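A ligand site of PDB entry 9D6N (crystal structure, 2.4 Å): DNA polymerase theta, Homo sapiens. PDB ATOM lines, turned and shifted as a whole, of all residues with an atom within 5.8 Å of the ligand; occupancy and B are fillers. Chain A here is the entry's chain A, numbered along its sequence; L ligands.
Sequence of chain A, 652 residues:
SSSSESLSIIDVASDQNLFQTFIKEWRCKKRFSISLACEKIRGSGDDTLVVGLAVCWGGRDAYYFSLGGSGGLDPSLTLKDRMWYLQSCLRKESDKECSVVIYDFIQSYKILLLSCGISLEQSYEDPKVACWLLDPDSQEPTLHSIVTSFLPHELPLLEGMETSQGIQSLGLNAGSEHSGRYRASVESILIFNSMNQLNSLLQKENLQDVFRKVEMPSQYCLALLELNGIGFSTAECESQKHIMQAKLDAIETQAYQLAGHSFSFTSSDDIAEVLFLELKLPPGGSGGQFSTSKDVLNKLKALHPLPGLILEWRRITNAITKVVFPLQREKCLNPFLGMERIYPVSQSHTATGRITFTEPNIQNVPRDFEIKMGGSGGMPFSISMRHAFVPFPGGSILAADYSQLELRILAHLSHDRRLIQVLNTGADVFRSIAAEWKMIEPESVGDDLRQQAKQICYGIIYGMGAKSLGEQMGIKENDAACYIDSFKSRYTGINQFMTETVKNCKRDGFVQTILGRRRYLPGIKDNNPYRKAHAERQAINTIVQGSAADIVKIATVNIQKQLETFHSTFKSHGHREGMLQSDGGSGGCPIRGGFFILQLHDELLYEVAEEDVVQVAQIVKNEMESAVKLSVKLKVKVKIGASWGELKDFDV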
ATOM      1  N   LEU A 407     -11.988 -17.340  34.492  1.00  0.00           N
ATOM      2  CA  LEU A 407     -10.674 -16.899  34.036  1.00  0.00           C
ATOM      3  C   LEU A 407      -9.597 -17.912  34.376  1.00  0.00           C
ATOM      4  O   LEU A 407      -8.667 -18.115  33.586  1.00  0.00           O
ATOM      5  CB  LEU A 407     -10.342 -15.534  34.658  1.00  0.00           C
ATOM      6  CG  LEU A 407     -11.242 -14.371  34.248  1.00  0.00           C
ATOM      7  CD1 LEU A 407     -10.955 -13.164  35.123  1.00  0.00           C
ATOM      8  CD2 LEU A 407     -11.057 -14.031  32.784  1.00  0.00           C
ATOM      9  N   ARG A 418       0.450 -15.207  30.039  1.00  0.00           N
ATOM     10  CA  ARG A 418       0.151 -13.837  30.457  1.00  0.00           C
ATOM     11  C   ARG A 418      -1.095 -13.801  31.341  1.00  0.00           C
ATOM     12  O   ARG A 418      -1.097 -13.133  32.388  1.00  0.00           O
ATOM     13  CB  ARG A 418      -0.014 -12.917  29.238  1.00  0.00           C
ATOM     14  CG  ARG A 418      -0.249 -11.460  29.622  1.00  0.00           C
ATOM     15  CD  ARG A 418       0.001 -10.518  28.449  1.00  0.00           C
ATOM     16  NE  ARG A 418      -0.583  -9.207  28.702  1.00  0.00           N
ATOM     17  CZ  ARG A 418      -0.183  -8.083  28.121  1.00  0.00           C
ATOM     18  NH1 ARG A 418       0.808  -8.071  27.235  1.00  0.00           N
ATOM     19  NH2 ARG A 418      -0.785  -6.939  28.431  1.00  0.00           N
ATOM     20  N   LEU A 419      -2.142 -14.535  30.966  1.00  0.00           N
ATOM     21  CA  LEU A 419      -3.339 -14.607  31.795  1.00  0.00           C
ATOM     22  C   LEU A 419      -3.041 -15.229  33.150  1.00  0.00           C
ATOM     23  O   LEU A 419      -3.480 -14.729  34.188  1.00  0.00           O
ATOM     24  CB  LEU A 419      -4.434 -15.385  31.070  1.00  0.00           C
ATOM     25  CG  LEU A 419      -5.629 -15.836  31.921  1.00  0.00           C
ATOM     26  CD1 LEU A 419      -6.359 -14.642  32.535  1.00  0.00           C
ATOM     27  CD2 LEU A 419      -6.580 -16.683  31.102  1.00  0.00           C
ATOM     28  N   VAL A 422      -1.376 -12.566  35.224  1.00  0.00           N
ATOM     29  CA  VAL A 422      -2.321 -11.559  35.705  1.00  0.00           C
ATOM     30  C   VAL A 422      -3.132 -12.116  36.871  1.00  0.00           C
ATOM     31  O   VAL A 422      -3.474 -11.378  37.810  1.00  0.00           O
ATOM     32  CB  VAL A 422      -3.239 -11.090  34.560  1.00  0.00           C
ATOM     33  CG1 VAL A 422      -4.201 -10.036  35.049  1.00  0.00           C
ATOM     34  CG2 VAL A 422      -2.407 -10.535  33.417  1.00  0.00           C
ATOM     35  N   VAL A 429      -8.263  -7.273  37.308  1.00  0.00           N
ATOM     36  CA  VAL A 429      -8.284  -7.070  35.861  1.00  0.00           C
ATOM     37  C   VAL A 429      -9.312  -6.020  35.479  1.00  0.00           C
ATOM     38  O   VAL A 429      -9.048  -5.140  34.645  1.00  0.00           O
ATOM     39  CB  VAL A 429      -8.569  -8.401  35.144  1.00  0.00           C
ATOM     40  CG1 VAL A 429      -8.488  -8.215  33.632  1.00  0.00           C
ATOM     41  CG2 VAL A 429      -7.600  -9.463  35.604  1.00  0.00           C
ATOM     42  N   SER A 432      -8.239  -2.538  36.152  1.00  0.00           N
ATOM     43  CA  SER A 432      -7.174  -2.154  35.244  1.00  0.00           C
ATOM     44  C   SER A 432      -7.698  -1.926  33.832  1.00  0.00           C
ATOM     45  O   SER A 432      -7.094  -1.149  33.072  1.00  0.00           O
ATOM     46  CB  SER A 432      -6.071  -3.217  35.227  1.00  0.00           C
ATOM     47  OG  SER A 432      -6.486  -4.364  34.514  1.00  0.00           O
ATOM     48  N   ILE A 433      -8.794  -2.587  33.457  1.00  0.00           N
ATOM     49  CA  ILE A 433      -9.383  -2.348  32.148  1.00  0.00           C
ATOM     50  C   ILE A 433     -10.007  -0.956  32.095  1.00  0.00           C
ATOM     51  O   ILE A 433      -9.847  -0.228  31.106  1.00  0.00           O
ATOM     52  CB  ILE A 433     -10.413  -3.442  31.821  1.00  0.00           C
ATOM     53  CG1 ILE A 433      -9.705  -4.770  31.582  1.00  0.00           C
ATOM     54  CG2 ILE A 433     -11.248  -3.058  30.607  1.00  0.00           C
ATOM     55  CD1 ILE A 433     -10.627  -5.888  31.263  1.00  0.00           C
ATOM     56  N   ALA A 434     -10.709  -0.559  33.154  1.00  0.00           N
ATOM     57  CA  ALA A 434     -11.281   0.777  33.207  1.00  0.00           C
ATOM     58  C   ALA A 434     -10.190   1.845  33.216  1.00  0.00           C
ATOM     59  O   ALA A 434     -10.384   2.929  32.653  1.00  0.00           O
ATOM     60  CB  ALA A 434     -12.177   0.920  34.437  1.00  0.00           C
ATOM     61  N   GLU A 436      -7.058   1.783  31.745  1.00  0.00           N
ATOM     62  CA  GLU A 436      -6.595   1.974  30.368  1.00  0.00           C
ATOM     63  C   GLU A 436      -7.700   2.545  29.487  1.00  0.00           C
ATOM     64  O   GLU A 436      -7.409   3.244  28.507  1.00  0.00           O
ATOM     65  CB  GLU A 436      -6.073   0.656  29.815  1.00  0.00           C
ATOM     66  CG  GLU A 436      -5.529   0.723  28.390  1.00  0.00           C
ATOM     67  CD  GLU A 436      -4.819  -0.557  27.967  1.00  0.00           C
ATOM     68  OE1 GLU A 436      -4.247  -1.233  28.839  1.00  0.00           O
ATOM     69  OE2 GLU A 436      -4.843  -0.881  26.756  1.00  0.00           O
ATOM     70  N   TRP A 437      -8.961   2.258  29.817  1.00  0.00           N
ATOM     71  CA  TRP A 437     -10.078   2.765  29.025  1.00  0.00           C
ATOM     72  C   TRP A 437     -10.302   4.252  29.285  1.00  0.00           C
ATOM     73  O   TRP A 437     -10.433   5.050  28.353  1.00  0.00           O
ATOM     74  CB  TRP A 437     -11.331   1.952  29.350  1.00  0.00           C
ATOM     75  CG  TRP A 437     -12.629   2.476  28.807  1.00  0.00           C
ATOM     76  CD1 TRP A 437     -12.828   3.290  27.730  1.00  0.00           C
ATOM     77  CD2 TRP A 437     -13.931   2.191  29.328  1.00  0.00           C
ATOM     78  NE1 TRP A 437     -14.165   3.540  27.553  1.00  0.00           N
ATOM     79  CE2 TRP A 437     -14.862   2.872  28.529  1.00  0.00           C
ATOM     80  CE3 TRP A 437     -14.401   1.426  30.401  1.00  0.00           C
ATOM     81  CZ2 TRP A 437     -16.240   2.810  28.761  1.00  0.00           C
ATOM     82  CZ3 TRP A 437     -15.755   1.369  30.635  1.00  0.00           C
ATOM     83  CH2 TRP A 437     -16.656   2.052  29.824  1.00  0.00           C
ATOM     84  N   ALA A 453     -16.468  -2.384  32.892  1.00  0.00           N
ATOM     85  CA  ALA A 453     -15.226  -2.996  32.428  1.00  0.00           C
ATOM     86  C   ALA A 453     -15.301  -4.517  32.485  1.00  0.00           C
ATOM     87  O   ALA A 453     -14.652  -5.202  31.690  1.00  0.00           O
ATOM     88  CB  ALA A 453     -14.048  -2.487  33.252  1.00  0.00           C
ATOM     89  N   ILE A 456     -17.057  -5.583  29.407  1.00  0.00           N
ATOM     90  CA  ILE A 456     -16.105  -5.381  28.314  1.00  0.00           C
ATOM     91  C   ILE A 456     -15.084  -6.509  28.275  1.00  0.00           C
ATOM     92  O   ILE A 456     -14.742  -7.021  27.200  1.00  0.00           O
ATOM     93  CB  ILE A 456     -15.416  -4.007  28.454  1.00  0.00           C
ATOM     94  CG1 ILE A 456     -16.416  -2.874  28.171  1.00  0.00           C
ATOM     95  CG2 ILE A 456     -14.209  -3.903  27.524  1.00  0.00           C
ATOM     96  CD1 ILE A 456     -15.872  -1.497  28.468  1.00  0.00           C
ATOM     97  N   CYS A 457     -14.622  -6.935  29.448  1.00  0.00           N
ATOM     98  CA  CYS A 457     -13.615  -8.001  29.524  1.00  0.00           C
ATOM     99  C   CYS A 457     -14.157  -9.305  28.947  1.00  0.00           C
ATOM    100  O   CYS A 457     -13.611  -9.855  27.981  1.00  0.00           O
ATOM    101  CB  CYS A 457     -13.176  -8.186  30.972  1.00  0.00           C
ATOM    102  SG  CYS A 457     -11.783  -9.310  31.179  1.00  0.00           S
ATOM    103  N   TYR A 458     -15.222  -9.834  29.547  1.00  0.00           N
ATOM    104  CA  TYR A 458     -15.764 -11.099  29.079  1.00  0.00           C
ATOM    105  C   TYR A 458     -16.355 -10.979  27.681  1.00  0.00           C
ATOM    106  O   TYR A 458     -16.343 -11.959  26.926  1.00  0.00           O
ATOM    107  CB  TYR A 458     -16.819 -11.614  30.065  1.00  0.00           C
ATOM    108  CG  TYR A 458     -16.263 -12.008  31.416  1.00  0.00           C
ATOM    109  CD1 TYR A 458     -15.328 -13.034  31.534  1.00  0.00           C
ATOM    110  CD2 TYR A 458     -16.667 -11.353  32.575  1.00  0.00           C
ATOM    111  CE1 TYR A 458     -14.813 -13.405  32.773  1.00  0.00           C
ATOM    112  CE2 TYR A 458     -16.155 -11.713  33.826  1.00  0.00           C
ATOM    113  CZ  TYR A 458     -15.227 -12.740  33.903  1.00  0.00           C
ATOM    114  OH  TYR A 458     -14.714 -13.101  35.132  1.00  0.00           O
ATOM    115  N   ILE A 460     -15.135  -9.134  25.058  1.00  0.00           N
ATOM    116  CA  ILE A 460     -14.026  -9.285  24.129  1.00  0.00           C
ATOM    117  C   ILE A 460     -13.527 -10.724  24.125  1.00  0.00           C
ATOM    118  O   ILE A 460     -13.274 -11.307  23.064  1.00  0.00           O
ATOM    119  CB  ILE A 460     -12.892  -8.296  24.476  1.00  0.00           C
ATOM    120  CG1 ILE A 460     -13.346  -6.854  24.213  1.00  0.00           C
ATOM    121  CG2 ILE A 460     -11.631  -8.625  23.697  1.00  0.00           C
ATOM    122  CD1 ILE A 460     -12.412  -5.805  24.762  1.00  0.00           C
ATOM    123  N   ILE A 461     -13.371 -11.326  25.312  1.00  0.00           N
ATOM    124  CA  ILE A 461     -12.874 -12.695  25.418  1.00  0.00           C
ATOM    125  C   ILE A 461     -13.783 -13.661  24.665  1.00  0.00           C
ATOM    126  O   ILE A 461     -13.303 -14.577  23.978  1.00  0.00           O
ATOM    127  CB  ILE A 461     -12.732 -13.088  26.897  1.00  0.00           C
ATOM    128  CG1 ILE A 461     -11.502 -12.421  27.509  1.00  0.00           C
ATOM    129  CG2 ILE A 461     -12.663 -14.604  27.057  1.00  0.00           C
ATOM    130  CD1 ILE A 461     -11.360 -12.650  28.993  1.00  0.00           C
ATOM    131  N   LEU A 469     -18.486  -3.123  20.848  1.00  0.00           N
ATOM    132  CA  LEU A 469     -17.513  -2.640  21.811  1.00  0.00           C
ATOM    133  C   LEU A 469     -17.383  -1.122  21.752  1.00  0.00           C
ATOM    134  O   LEU A 469     -17.160  -0.474  22.791  1.00  0.00           O
ATOM    135  CB  LEU A 469     -16.162  -3.302  21.582  1.00  0.00           C
ATOM    136  CG  LEU A 469     -15.056  -2.880  22.553  1.00  0.00           C
ATOM    137  CD1 LEU A 469     -15.415  -3.276  23.980  1.00  0.00           C
ATOM    138  CD2 LEU A 469     -13.725  -3.488  22.138  1.00  0.00           C
ATOM    139  N   MET A 473     -18.110   1.491  24.771  1.00  0.00           N
ATOM    140  CA  MET A 473     -17.011   2.321  25.236  1.00  0.00           C
ATOM    141  C   MET A 473     -17.167   3.791  24.872  1.00  0.00           C
ATOM    142  O   MET A 473     -16.342   4.608  25.277  1.00  0.00           O
ATOM    143  CB  MET A 473     -15.681   1.807  24.683  1.00  0.00           C
ATOM    144  CG  MET A 473     -15.253   0.454  25.252  1.00  0.00           C
ATOM    145  SD  MET A 473     -13.720  -0.160  24.526  1.00  0.00           S
ATOM    146  CE  MET A 473     -12.497   0.871  25.323  1.00  0.00           C
ATOM    147  N   CYS A 482      -8.948  -1.505  17.711  1.00  0.00           N
ATOM    148  CA  CYS A 482      -7.582  -1.502  18.229  1.00  0.00           C
ATOM    149  C   CYS A 482      -7.511  -2.196  19.589  1.00  0.00           C
ATOM    150  O   CYS A 482      -6.524  -2.882  19.889  1.00  0.00           O
ATOM    151  CB  CYS A 482      -7.053  -0.074  18.327  1.00  0.00           C
ATOM    152  SG  CYS A 482      -7.063   0.817  16.752  1.00  0.00           S
ATOM    153  N   TYR A 483      -8.539  -2.018  20.430  1.00  0.00           N
ATOM    154  CA  TYR A 483      -8.560  -2.695  21.721  1.00  0.00           C
ATOM    155  C   TYR A 483      -8.688  -4.210  21.541  1.00  0.00           C
ATOM    156  O   TYR A 483      -8.023  -4.981  22.242  1.00  0.00           O
ATOM    157  CB  TYR A 483      -9.714  -2.169  22.579  1.00  0.00           C
ATOM    158  CG  TYR A 483      -9.528  -0.750  23.058  1.00  0.00           C
ATOM    159  CD1 TYR A 483      -8.795  -0.477  24.212  1.00  0.00           C
ATOM    160  CD2 TYR A 483     -10.088   0.317  22.375  1.00  0.00           C
ATOM    161  CE1 TYR A 483      -8.630   0.822  24.664  1.00  0.00           C
ATOM    162  CE2 TYR A 483      -9.925   1.626  22.817  1.00  0.00           C
ATOM    163  CZ  TYR A 483      -9.202   1.870  23.964  1.00  0.00           C
ATOM    164  OH  TYR A 483      -9.034   3.156  24.403  1.00  0.00           O
ATOM    165  N   ILE A 484      -9.539  -4.646  20.604  1.00  0.00           N
ATOM    166  CA  ILE A 484      -9.688  -6.069  20.348  1.00  0.00           C
ATOM    167  C   ILE A 484      -8.386  -6.649  19.795  1.00  0.00           C
ATOM    168  O   ILE A 484      -7.902  -7.683  20.251  1.00  0.00           O
ATOM    169  CB  ILE A 484     -10.870  -6.329  19.391  1.00  0.00           C
ATOM    170  CG1 ILE A 484     -12.177  -5.885  20.041  1.00  0.00           C
ATOM    171  CG2 ILE A 484     -10.929  -7.791  19.000  1.00  0.00           C
ATOM    172  CD1 ILE A 484     -13.387  -6.042  19.141  1.00  0.00           C
ATOM    173  N   SER A 486      -5.410  -5.552  20.161  1.00  0.00           N
ATOM    174  CA  SER A 486      -4.379  -5.571  21.195  1.00  0.00           C
ATOM    175  C   SER A 486      -4.535  -6.757  22.129  1.00  0.00           C
ATOM    176  O   SER A 486      -3.551  -7.385  22.518  1.00  0.00           O
ATOM    177  CB  SER A 486      -4.404  -4.268  21.986  1.00  0.00           C
ATOM    178  OG  SER A 486      -3.578  -4.366  23.135  1.00  0.00           O
ATOM    179  N   PHE A 487      -5.780  -7.086  22.495  1.00  0.00           N
ATOM    180  CA  PHE A 487      -6.020  -8.236  23.366  1.00  0.00           C
ATOM    181  C   PHE A 487      -5.529  -9.522  22.719  1.00  0.00           C
ATOM    182  O   PHE A 487      -4.856 -10.340  23.361  1.00  0.00           O
ATOM    183  CB  PHE A 487      -7.513  -8.347  23.700  1.00  0.00           C
ATOM    184  CG  PHE A 487      -7.890  -9.669  24.298  1.00  0.00           C
ATOM    185  CD1 PHE A 487      -7.615  -9.949  25.628  1.00  0.00           C
ATOM    186  CD2 PHE A 487      -8.514 -10.638  23.536  1.00  0.00           C
ATOM    187  CE1 PHE A 487      -7.951 -11.171  26.180  1.00  0.00           C
ATOM    188  CE2 PHE A 487      -8.855 -11.860  24.079  1.00  0.00           C
ATOM    189  CZ  PHE A 487      -8.577 -12.130  25.408  1.00  0.00           C
ATOM    190  N   ARG A 490      -1.766  -9.551  22.915  1.00  0.00           N
ATOM    191  CA  ARG A 490      -1.238  -9.784  24.260  1.00  0.00           C
ATOM    192  C   ARG A 490      -1.481 -11.219  24.714  1.00  0.00           C
ATOM    193  O   ARG A 490      -0.651 -11.779  25.439  1.00  0.00           O
ATOM    194  CB  ARG A 490      -1.863  -8.813  25.258  1.00  0.00           C
ATOM    195  CG  ARG A 490      -1.611  -7.337  24.985  1.00  0.00           C
ATOM    196  CD  ARG A 490      -2.550  -6.462  25.796  1.00  0.00           C
ATOM    197  NE  ARG A 490      -2.228  -5.041  25.699  1.00  0.00           N
ATOM    198  CZ  ARG A 490      -2.814  -4.099  26.409  1.00  0.00           C
ATOM    199  NH1 ARG A 490      -3.806  -4.382  27.245  1.00  0.00           N
ATOM    200  NH2 ARG A 490      -2.405  -2.833  26.294  1.00  0.00           N
ATOM    201  N   TYR A 491      -2.602 -11.814  24.318  1.00  0.00           N
ATOM    202  CA  TYR A 491      -3.047 -13.094  24.860  1.00  0.00           C
ATOM    203  C   TYR A 491      -3.188 -14.097  23.702  1.00  0.00           C
ATOM    204  O   TYR A 491      -4.305 -14.447  23.300  1.00  0.00           O
ATOM    205  CB  TYR A 491      -4.361 -12.927  25.635  1.00  0.00           C
ATOM    206  CG  TYR A 491      -4.200 -12.057  26.868  1.00  0.00           C
ATOM    207  CD1 TYR A 491      -3.854 -12.617  28.085  1.00  0.00           C
ATOM    208  CD2 TYR A 491      -4.369 -10.687  26.799  1.00  0.00           C
ATOM    209  CE1 TYR A 491      -3.698 -11.825  29.221  1.00  0.00           C
ATOM    210  CE2 TYR A 491      -4.218  -9.884  27.916  1.00  0.00           C
ATOM    211  CZ  TYR A 491      -3.869 -10.456  29.121  1.00  0.00           C
ATOM    212  OH  TYR A 491      -3.721  -9.663  30.238  1.00  0.00           O
ATOM    213  N   ILE A 494      -4.695 -17.617  24.778  1.00  0.00           N
ATOM    214  CA  ILE A 494      -6.153 -17.627  24.764  1.00  0.00           C
ATOM    215  C   ILE A 494      -6.677 -17.678  23.334  1.00  0.00           C
ATOM    216  O   ILE A 494      -7.618 -18.420  23.033  1.00  0.00           O
ATOM    217  CB  ILE A 494      -6.701 -16.392  25.520  1.00  0.00           C
ATOM    218  CG1 ILE A 494      -6.343 -16.474  27.004  1.00  0.00           C
ATOM    219  CG2 ILE A 494      -8.202 -16.270  25.321  1.00  0.00           C
ATOM    220  CD1 ILE A 494      -6.639 -15.204  27.754  1.00  0.00           C
HETATM  221  C1  LIG L   1      -8.712  -7.990  28.534  1.00  0.00           C
HETATM  222  C2  LIG L   1      -6.689  -8.336  30.482  1.00  0.00           C
HETATM  223  C3  LIG L   1      -4.552  -5.943  30.026  1.00  0.00           C
HETATM  224  C4  LIG L   1      -7.567  -9.381  30.169  1.00  0.00           C
HETATM  225  C5  LIG L   1      -7.448 -10.697  30.855  1.00  0.00           C
HETATM  226  C6  LIG L   1       0.329  -5.217  33.243  1.00  0.00           C
HETATM  227  C7  LIG L   1      -2.036  -4.639  31.746  1.00  0.00           C
HETATM  228  C8  LIG L   1      -7.817  -6.947  28.862  1.00  0.00           C
HETATM  229  C9  LIG L   1      -7.042  -5.512  27.181  1.00  0.00           C
HETATM  230  C10 LIG L   1      -6.459  -4.146  25.058  1.00  0.00           C
HETATM  231  C11 LIG L   1      -8.306  -3.475  26.619  1.00  0.00           C
HETATM  232  C12 LIG L   1      -9.565  -3.592  26.000  1.00  0.00           C
HETATM  233  C13 LIG L   1     -10.581  -2.719  26.367  1.00  0.00           C
HETATM  234  C14 LIG L   1     -10.355  -1.747  27.348  1.00  0.00           C
HETATM  235  C15 LIG L   1      -9.122  -1.646  27.966  1.00  0.00           C
HETATM  236  C16 LIG L   1      -8.097  -2.520  27.596  1.00  0.00           C
HETATM  237  C17 LIG L   1      -6.809  -7.120  29.826  1.00  0.00           C
HETATM  238  C18 LIG L   1      -6.431  -4.736  30.628  1.00  0.00           C
HETATM  239  C19 LIG L   1      -5.253  -3.827  30.835  1.00  0.00           C
HETATM  240  C20 LIG L   1      -2.754  -4.183  30.474  1.00  0.00           C
HETATM  241  C21 LIG L   1      -1.097  -5.824  31.360  1.00  0.00           C
HETATM  242  C22 LIG L   1      -0.964  -7.260  33.347  1.00  0.00           C
HETATM  243  C23 LIG L   1      -8.561  -9.191  29.199  1.00  0.00           C
HETATM  244  C24 LIG L   1      -9.801  -7.783  27.486  1.00  0.00           C
HETATM  245  F1  LIG L   1     -11.370  -0.897  27.703  1.00  0.00           F
HETATM  246  F2  LIG L   1      -8.687 -11.041  31.326  1.00  0.00           F
HETATM  247  F3  LIG L   1      -6.580 -10.596  31.906  1.00  0.00           F
HETATM  248  F4  LIG L   1      -7.013 -11.637  29.969  1.00  0.00           F
HETATM  249  F5  LIG L   1     -10.457  -8.956  27.251  1.00  0.00           F
HETATM  250  F6  LIG L   1      -9.274  -7.326  26.316  1.00  0.00           F
HETATM  251  F7  LIG L   1     -10.687  -6.852  27.941  1.00  0.00           F
HETATM  252  N1  LIG L   1      -7.256  -4.375  26.270  1.00  0.00           N
HETATM  253  N2  LIG L   1      -5.931  -6.014  30.129  1.00  0.00           N
HETATM  254  N3  LIG L   1      -4.163  -4.689  30.427  1.00  0.00           N
HETATM  255  N4  LIG L   1      -0.246  -6.322  32.467  1.00  0.00           N
HETATM  256  O1  LIG L   1      -6.123  -6.243  27.053  1.00  0.00           O
HETATM  257  O2  LIG L   1      -7.949  -5.690  28.180  1.00  0.00           O
HETATM  258  O3  LIG L   1      -3.024  -5.080  32.685  1.00  0.00           O
HETATM  259  O4  LIG L   1      -3.828  -6.833  29.639  1.00  0.00           O
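An oxygen (O4) of the ligand lies within hydrogen-bond range of the side-chain hydroxyl (OH) of Tyr 491 (2.9 Å). The guanidinium group of Arg 490 is in hydrogen-bond range of an oxygen (O1) of the ligand. An oxygen (O4) of the ligand sits close to the guanidinium group (NH2) of Arg 418, at 3.3 Å.
The guanidinium group of Arg 490 lies within salt-bridge range of the side-chain carboxylate of Glu 436, 3.2 Å away. NE of Arg 490 lies within hydrogen-bond range of OG of Ser 486 (3.0 Å). The indole nitrogen of Trp 437 is in hydrogen-bond range of the backbone carbonyl oxygen of Met 473 (3.3 Å). The backbone carbonyl oxygen (O) of Val 429 lies within hydrogen-bond range of the side-chain hydroxyl (OG) of Ser 432.
The backbone carbonyl oxygen (O) of Cys 457 sits close to a fluorine (F5) of the ligand, 3.4 Å away. Merely in contact with the ligand: Met 473 (3.2 Å), Phe 487 (3.2 Å), Trp 437 (3.3 Å), Tyr 483 (3.3 Å), Ile 433 (3.4 Å), Glu 436 (3.4 Å), Ser 486 (3.5 Å), Val 429 (3.5 Å), Val 422 (3.6 Å), Ile 461 (3.6 Å), Ile 460 (3.8 Å), Ser 432 (3.9 Å) and Ile 456 (3.99 Å). Hydrophobic or aromatic side chains that line the ligand: Val 422, Val 429, Ile 433, Trp 437, Ile 456, Ile 460, Ile 461, Met 473, Tyr 483, Phe 487 and Tyr 491. Within 4 Å of the ligand: Arg 418, Val 422, Val 429, Ser 432, Ile 433, Glu 436, Trp 437, Ile 456, Cys 457, Ile 460, Ile 461, Met 473, Tyr 483, Ser 486, Phe 487, Arg 490 and Tyr 491.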
